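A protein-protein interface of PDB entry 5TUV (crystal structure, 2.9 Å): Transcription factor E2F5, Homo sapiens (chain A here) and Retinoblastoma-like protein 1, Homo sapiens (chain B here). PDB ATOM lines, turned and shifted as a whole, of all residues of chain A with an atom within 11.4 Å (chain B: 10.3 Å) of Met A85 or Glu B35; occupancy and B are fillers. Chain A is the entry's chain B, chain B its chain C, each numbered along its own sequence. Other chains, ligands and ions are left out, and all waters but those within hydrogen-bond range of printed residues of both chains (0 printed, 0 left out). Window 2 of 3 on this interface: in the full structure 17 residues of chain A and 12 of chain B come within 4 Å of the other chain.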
ATOM      1  N   PRO A  81     -15.965  15.347 -21.201  1.00  0.00           N
ATOM      2  CA  PRO A  81     -16.743  14.107 -21.244  1.00  0.00           C
ATOM      3  C   PRO A  81     -15.858  12.866 -21.242  1.00  0.00           C
ATOM      4  O   PRO A  81     -14.648  12.960 -21.444  1.00  0.00           O
ATOM      5  CB  PRO A  81     -17.509  14.226 -22.560  1.00  0.00           C
ATOM      6  CG  PRO A  81     -16.616  15.037 -23.422  1.00  0.00           C
ATOM      7  CD  PRO A  81     -15.939  16.026 -22.508  1.00  0.00           C
ATOM      8  N   ILE A  82     -16.475  11.714 -21.008  1.00  0.00           N
ATOM      9  CA  ILE A  82     -15.770  10.440 -21.001  1.00  0.00           C
ATOM     10  C   ILE A  82     -15.291  10.041 -22.399  1.00  0.00           C
ATOM     11  O   ILE A  82     -15.968  10.296 -23.394  1.00  0.00           O
ATOM     12  CB  ILE A  82     -16.654   9.316 -20.388  1.00  0.00           C
ATOM     13  CG1 ILE A  82     -18.150   9.546 -20.656  1.00  0.00           C
ATOM     14  CG2 ILE A  82     -16.442   9.239 -18.888  1.00  0.00           C
ATOM     15  CD1 ILE A  82     -18.586   9.523 -22.107  1.00  0.00           C
ATOM     16  N   PRO A  83     -14.092   9.447 -22.480  1.00  0.00           N
ATOM     17  CA  PRO A  83     -13.562   9.007 -23.774  1.00  0.00           C
ATOM     18  C   PRO A  83     -14.336   7.823 -24.359  1.00  0.00           C
ATOM     19  O   PRO A  83     -13.778   6.732 -24.479  1.00  0.00           O
ATOM     20  CB  PRO A  83     -12.122   8.598 -23.440  1.00  0.00           C
ATOM     21  CG  PRO A  83     -11.792   9.359 -22.196  1.00  0.00           C
ATOM     22  CD  PRO A  83     -13.075   9.359 -21.419  1.00  0.00           C
ATOM     23  N   GLU A  84     -15.586   8.050 -24.752  1.00  0.00           N
ATOM     24  CA  GLU A  84     -16.399   6.998 -25.358  1.00  0.00           C
ATOM     25  C   GLU A  84     -15.977   6.827 -26.806  1.00  0.00           C
ATOM     26  O   GLU A  84     -15.012   7.441 -27.247  1.00  0.00           O
ATOM     27  CB  GLU A  84     -17.891   7.338 -25.289  1.00  0.00           C
ATOM     28  CG  GLU A  84     -18.676   6.635 -24.194  1.00  0.00           C
ATOM     29  CD  GLU A  84     -20.095   7.167 -24.074  1.00  0.00           C
ATOM     30  OE1 GLU A  84     -20.469   8.046 -24.879  1.00  0.00           O
ATOM     31  OE2 GLU A  84     -20.832   6.709 -23.176  1.00  0.00           O
ATOM     32  N   MET A  85     -16.695   5.988 -27.545  1.00  0.00           N
ATOM     33  CA  MET A  85     -16.418   5.819 -28.965  1.00  0.00           C
ATOM     34  C   MET A  85     -17.673   6.077 -29.788  1.00  0.00           C
ATOM     35  O   MET A  85     -18.778   5.721 -29.379  1.00  0.00           O
ATOM     36  CB  MET A  85     -15.870   4.420 -29.253  1.00  0.00           C
ATOM     37  CG  MET A  85     -15.051   4.337 -30.534  1.00  0.00           C
ATOM     38  SD  MET A  85     -13.717   3.124 -30.449  1.00  0.00           S
ATOM     39  CE  MET A  85     -13.077   3.199 -32.122  1.00  0.00           C
ATOM     40  N   GLY A  86     -17.497   6.706 -30.946  1.00  0.00           N
ATOM     41  CA  GLY A  86     -18.615   7.033 -31.810  1.00  0.00           C
ATOM     42  C   GLY A  86     -18.422   6.527 -33.226  1.00  0.00           C
ATOM     43  O   GLY A  86     -19.134   5.629 -33.676  1.00  0.00           O
ATOM     44  N   GLN A  90     -14.275   6.344 -33.861  1.00  0.00           N
ATOM     45  CA  GLN A  90     -13.108   6.749 -33.088  1.00  0.00           C
ATOM     46  C   GLN A  90     -13.514   7.329 -31.738  1.00  0.00           C
ATOM     47  O   GLN A  90     -14.623   7.838 -31.579  1.00  0.00           O
ATOM     48  CB  GLN A  90     -12.277   7.773 -33.866  1.00  0.00           C
ATOM     49  N   LYS A  91     -12.606   7.248 -30.771  1.00  0.00           N
ATOM     50  CA  LYS A  91     -12.872   7.752 -29.431  1.00  0.00           C
ATOM     51  C   LYS A  91     -12.908   9.270 -29.492  1.00  0.00           C
ATOM     52  O   LYS A  91     -12.331   9.868 -30.401  1.00  0.00           O
ATOM     53  CB  LYS A  91     -11.806   7.296 -28.433  1.00  0.00           C
ATOM     54  CG  LYS A  91     -11.258   5.900 -28.645  1.00  0.00           C
ATOM     55  CD  LYS A  91     -10.224   5.579 -27.572  1.00  0.00           C
ATOM     56  CE  LYS A  91     -10.838   4.995 -26.312  1.00  0.00           C
ATOM     57  NZ  LYS A  91      -9.889   4.093 -25.601  1.00  0.00           N
ATOM     58  N   LYS A  92     -13.566   9.902 -28.528  1.00  0.00           N
ATOM     59  CA  LYS A  92     -13.647  11.354 -28.546  1.00  0.00           C
ATOM     60  C   LYS A  92     -12.954  11.964 -27.329  1.00  0.00           C
ATOM     61  O   LYS A  92     -13.306  11.698 -26.179  1.00  0.00           O
ATOM     62  CB  LYS A  92     -15.114  11.821 -28.642  1.00  0.00           C
ATOM     63  CG  LYS A  92     -15.968  11.646 -27.385  1.00  0.00           C
ATOM     64  CD  LYS A  92     -17.357  12.246 -27.552  1.00  0.00           C
ATOM     65  CE  LYS A  92     -18.202  12.035 -26.303  1.00  0.00           C
ATOM     66  NZ  LYS A  92     -19.652  12.271 -26.551  1.00  0.00           N
ATOM     67  N   TYR A  93     -11.907  12.735 -27.599  1.00  0.00           N
ATOM     68  CA  TYR A  93     -11.250  13.481 -26.542  1.00  0.00           C
ATOM     69  C   TYR A  93     -11.552  14.942 -26.807  1.00  0.00           C
ATOM     70  O   TYR A  93     -11.041  15.524 -27.764  1.00  0.00           O
ATOM     71  CB  TYR A  93      -9.740  13.231 -26.532  1.00  0.00           C
ATOM     72  CG  TYR A  93      -9.344  11.776 -26.421  1.00  0.00           C
ATOM     73  CD1 TYR A  93      -9.324  11.133 -25.191  1.00  0.00           C
ATOM     74  CD2 TYR A  93      -8.975  11.050 -27.547  1.00  0.00           C
ATOM     75  CE1 TYR A  93      -8.958   9.804 -25.086  1.00  0.00           C
ATOM     76  CE2 TYR A  93      -8.607   9.721 -27.452  1.00  0.00           C
ATOM     77  CZ  TYR A  93      -8.599   9.103 -26.219  1.00  0.00           C
ATOM     78  OH  TYR A  93      -8.234   7.780 -26.118  1.00  0.00           O
ATOM     79  N   GLN A  94     -12.384  15.539 -25.964  1.00  0.00           N
ATOM     80  CA  GLN A  94     -12.758  16.930 -26.160  1.00  0.00           C
ATOM     81  C   GLN A  94     -12.809  17.724 -24.864  1.00  0.00           C
ATOM     82  O   GLN A  94     -12.813  17.164 -23.767  1.00  0.00           O
ATOM     83  CB  GLN A  94     -14.095  17.040 -26.899  1.00  0.00           C
ATOM     84  CG  GLN A  94     -15.158  16.049 -26.497  1.00  0.00           C
ATOM     85  CD  GLN A  94     -16.477  16.327 -27.191  1.00  0.00           C
ATOM     86  OE1 GLN A  94     -17.348  17.005 -26.647  1.00  0.00           O
ATOM     87  NE2 GLN A  94     -16.624  15.815 -28.409  1.00  0.00           N
ATOM     88  N   SER B  10     -22.387  12.873 -16.533  1.00  0.00           N
ATOM     89  CA  SER B  10     -21.672  12.037 -17.490  1.00  0.00           C
ATOM     90  C   SER B  10     -20.338  12.663 -17.880  1.00  0.00           C
ATOM     91  O   SER B  10     -19.690  12.226 -18.832  1.00  0.00           O
ATOM     92  CB  SER B  10     -22.526  11.800 -18.737  1.00  0.00           C
ATOM     93  OG  SER B  10     -21.830  11.019 -19.692  1.00  0.00           O
ATOM     94  N   ASN B  29      -6.779  11.461 -15.173  1.00  0.00           N
ATOM     95  CA  ASN B  29      -6.845  10.018 -14.973  1.00  0.00           C
ATOM     96  C   ASN B  29      -7.945   9.376 -15.811  1.00  0.00           C
ATOM     97  O   ASN B  29      -7.765   8.286 -16.355  1.00  0.00           O
ATOM     98  CB  ASN B  29      -7.062   9.690 -13.494  1.00  0.00           C
ATOM     99  CG  ASN B  29      -5.834   9.966 -12.650  1.00  0.00           C
ATOM    100  OD1 ASN B  29      -4.713  10.010 -13.158  1.00  0.00           O
ATOM    101  ND2 ASN B  29      -6.037  10.149 -11.351  1.00  0.00           N
ATOM    102  N   MET B  30      -9.080  10.059 -15.912  1.00  0.00           N
ATOM    103  CA  MET B  30     -10.212   9.567 -16.690  1.00  0.00           C
ATOM    104  C   MET B  30      -9.856   9.458 -18.170  1.00  0.00           C
ATOM    105  O   MET B  30     -10.176   8.465 -18.823  1.00  0.00           O
ATOM    106  CB  MET B  30     -11.423  10.483 -16.510  1.00  0.00           C
ATOM    107  CG  MET B  30     -12.657  10.037 -17.276  1.00  0.00           C
ATOM    108  SD  MET B  30     -13.919  11.323 -17.363  1.00  0.00           S
ATOM    109  CE  MET B  30     -13.055  12.580 -18.300  1.00  0.00           C
ATOM    110  N   ILE B  31      -9.193  10.486 -18.688  1.00  0.00           N
ATOM    111  CA  ILE B  31      -8.783  10.519 -20.087  1.00  0.00           C
ATOM    112  C   ILE B  31      -7.762   9.428 -20.391  1.00  0.00           C
ATOM    113  O   ILE B  31      -7.838   8.757 -21.421  1.00  0.00           O
ATOM    114  CB  ILE B  31      -8.190  11.893 -20.462  1.00  0.00           C
ATOM    115  CG1 ILE B  31      -9.253  12.983 -20.325  1.00  0.00           C
ATOM    116  CG2 ILE B  31      -7.637  11.875 -21.878  1.00  0.00           C
ATOM    117  CD1 ILE B  31     -10.475  12.747 -21.181  1.00  0.00           C
ATOM    118  N   ARG B  32      -6.815   9.244 -19.477  1.00  0.00           N
ATOM    119  CA  ARG B  32      -5.744   8.274 -19.667  1.00  0.00           C
ATOM    120  C   ARG B  32      -6.244   6.834 -19.555  1.00  0.00           C
ATOM    121  O   ARG B  32      -5.745   5.942 -20.243  1.00  0.00           O
ATOM    122  CB  ARG B  32      -4.626   8.522 -18.652  1.00  0.00           C
ATOM    123  CG  ARG B  32      -3.394   7.661 -18.857  1.00  0.00           C
ATOM    124  CD  ARG B  32      -2.362   7.932 -17.779  1.00  0.00           C
ATOM    125  NE  ARG B  32      -2.967   7.948 -16.451  1.00  0.00           N
ATOM    126  CZ  ARG B  32      -3.256   6.859 -15.747  1.00  0.00           C
ATOM    127  NH1 ARG B  32      -2.998   5.657 -16.242  1.00  0.00           N
ATOM    128  NH2 ARG B  32      -3.807   6.972 -14.546  1.00  0.00           N
ATOM    129  N   GLN B  33      -7.230   6.610 -18.692  1.00  0.00           N
ATOM    130  CA  GLN B  33      -7.775   5.270 -18.491  1.00  0.00           C
ATOM    131  C   GLN B  33      -8.890   4.946 -19.482  1.00  0.00           C
ATOM    132  O   GLN B  33      -8.913   3.863 -20.069  1.00  0.00           O
ATOM    133  CB  GLN B  33      -8.293   5.112 -17.061  1.00  0.00           C
ATOM    134  CG  GLN B  33      -7.202   4.893 -16.026  1.00  0.00           C
ATOM    135  CD  GLN B  33      -7.760   4.627 -14.642  1.00  0.00           C
ATOM    136  OE1 GLN B  33      -8.603   5.373 -14.145  1.00  0.00           O
ATOM    137  NE2 GLN B  33      -7.295   3.552 -14.013  1.00  0.00           N
ATOM    138  N   GLY B  34      -9.813   5.885 -19.664  1.00  0.00           N
ATOM    139  CA  GLY B  34     -10.940   5.679 -20.555  1.00  0.00           C
ATOM    140  C   GLY B  34     -12.007   4.804 -19.926  1.00  0.00           C
ATOM    141  O   GLY B  34     -12.121   4.737 -18.702  1.00  0.00           O
ATOM    142  N   GLU B  35     -12.792   4.131 -20.763  1.00  0.00           N
ATOM    143  CA  GLU B  35     -13.845   3.247 -20.277  1.00  0.00           C
ATOM    144  C   GLU B  35     -13.253   2.020 -19.590  1.00  0.00           C
ATOM    145  O   GLU B  35     -12.363   1.361 -20.128  1.00  0.00           O
ATOM    146  CB  GLU B  35     -14.763   2.821 -21.424  1.00  0.00           C
ATOM    147  CG  GLU B  35     -15.353   3.983 -22.208  1.00  0.00           C
ATOM    148  CD  GLU B  35     -16.359   3.532 -23.249  1.00  0.00           C
ATOM    149  OE1 GLU B  35     -17.376   2.916 -22.867  1.00  0.00           O
ATOM    150  OE2 GLU B  35     -16.133   3.792 -24.451  1.00  0.00           O
ATOM    151  N   GLN B  36     -13.755   1.720 -18.396  1.00  0.00           N
ATOM    152  CA  GLN B  36     -13.217   0.633 -17.587  1.00  0.00           C
ATOM    153  C   GLN B  36     -14.177  -0.547 -17.490  1.00  0.00           C
ATOM    154  O   GLN B  36     -15.393  -0.382 -17.587  1.00  0.00           O
ATOM    155  CB  GLN B  36     -12.881   1.139 -16.182  1.00  0.00           C
ATOM    156  CG  GLN B  36     -11.834   2.238 -16.148  1.00  0.00           C
ATOM    157  CD  GLN B  36     -10.420   1.694 -16.157  1.00  0.00           C
ATOM    158  OE1 GLN B  36      -9.729   1.744 -17.175  1.00  0.00           O
ATOM    159  NE2 GLN B  36      -9.979   1.174 -15.018  1.00  0.00           N
ATOM    160  N   ARG B  37     -13.622  -1.740 -17.299  1.00  0.00           N
ATOM    161  CA  ARG B  37     -14.428  -2.926 -17.042  1.00  0.00           C
ATOM    162  C   ARG B  37     -14.965  -2.881 -15.617  1.00  0.00           C
ATOM    163  O   ARG B  37     -14.294  -2.390 -14.710  1.00  0.00           O
ATOM    164  CB  ARG B  37     -13.613  -4.203 -17.261  1.00  0.00           C
ATOM    165  CG  ARG B  37     -13.234  -4.480 -18.708  1.00  0.00           C
ATOM    166  CD  ARG B  37     -12.465  -5.789 -18.819  1.00  0.00           C
ATOM    167  NE  ARG B  37     -11.834  -5.955 -20.125  1.00  0.00           N
ATOM    168  CZ  ARG B  37     -12.221  -6.844 -21.034  1.00  0.00           C
ATOM    169  NH1 ARG B  37     -13.236  -7.654 -20.779  1.00  0.00           N
ATOM    170  NH2 ARG B  37     -11.589  -6.924 -22.197  1.00  0.00           N
ATOM    171  N   THR B  38     -16.176  -3.394 -15.420  1.00  0.00           N
ATOM    172  CA  THR B  38     -16.802  -3.375 -14.103  1.00  0.00           C
ATOM    173  C   THR B  38     -16.331  -4.546 -13.248  1.00  0.00           C
ATOM    174  O   THR B  38     -17.129  -5.393 -12.845  1.00  0.00           O
ATOM    175  CB  THR B  38     -18.337  -3.414 -14.208  1.00  0.00           C
ATOM    176  OG1 THR B  38     -18.769  -4.751 -14.485  1.00  0.00           O
ATOM    177  CG2 THR B  38     -18.821  -2.482 -15.309  1.00  0.00           C
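Hydrophobic or aromatic side chains of chain B within 4 Å of the printed part of chain A: Met B30 and Ile B31.
Hydrophobic or aromatic side chains of chain A within 4 Å of the printed part of chain B: Ile A82, Pro A83 and Tyr A93.
Among the printed residues, 9 pairs touch across the chains.
Among the printed residues, no Asp or Glu carboxylate lies within 4 Å of a Lys or Arg side-chain nitrogen of the other chain.
O of Glu A84 sits at hydrogen-bond distance from N of Lys A92 (3.1 Å).
Of the printed residues of chain B, Met A85 touches Glu B35 (3.8 Å).
No residue of chain B comes within 4 Å of Gly A86.
Gln A90 touches none of the printed residues of chain B.
No residue of chain B comes within 4 Å of Lys A91.
No residue of chain A comes within 4 Å of Gly B34.
No residue of chain A comes within 4 Å of Gln B36.
Printed residues of chain B within 4 Å of Ile A82: Ser B10 (3.6 Å) and Met B30 (3.6 Å).
Printed residues of chain B within 4 Å of Pro A81: Met B30.
Of the printed residues of chain A, Met B30 touches Pro A81 (3.5 Å), Ile A82 (3.6 Å) and Pro A83 (3.8 Å).
Arg B37 touches none of the printed residues of chain A.
The nearest residue of chain B that does not touch Met A85 is Gly B34 (9.0 Å).
Pro A81 touches Met B30.
Ser B10 touches Ile A82.
SD of Met B30 touches CG2 of Ile A82, 3.6 Å away.
CG of Pro A83 touches O of Met B30, 3.8 Å away.
Pro A83 touches Ile B31.
Pro A83 touches Glu B35 (O to OE2, 3.8 Å).
Glu A84 touches Glu B35.
Met A85 touches Glu B35.
Tyr A93 touches Ile B31 (CD1 to CG2, 3.8 Å).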
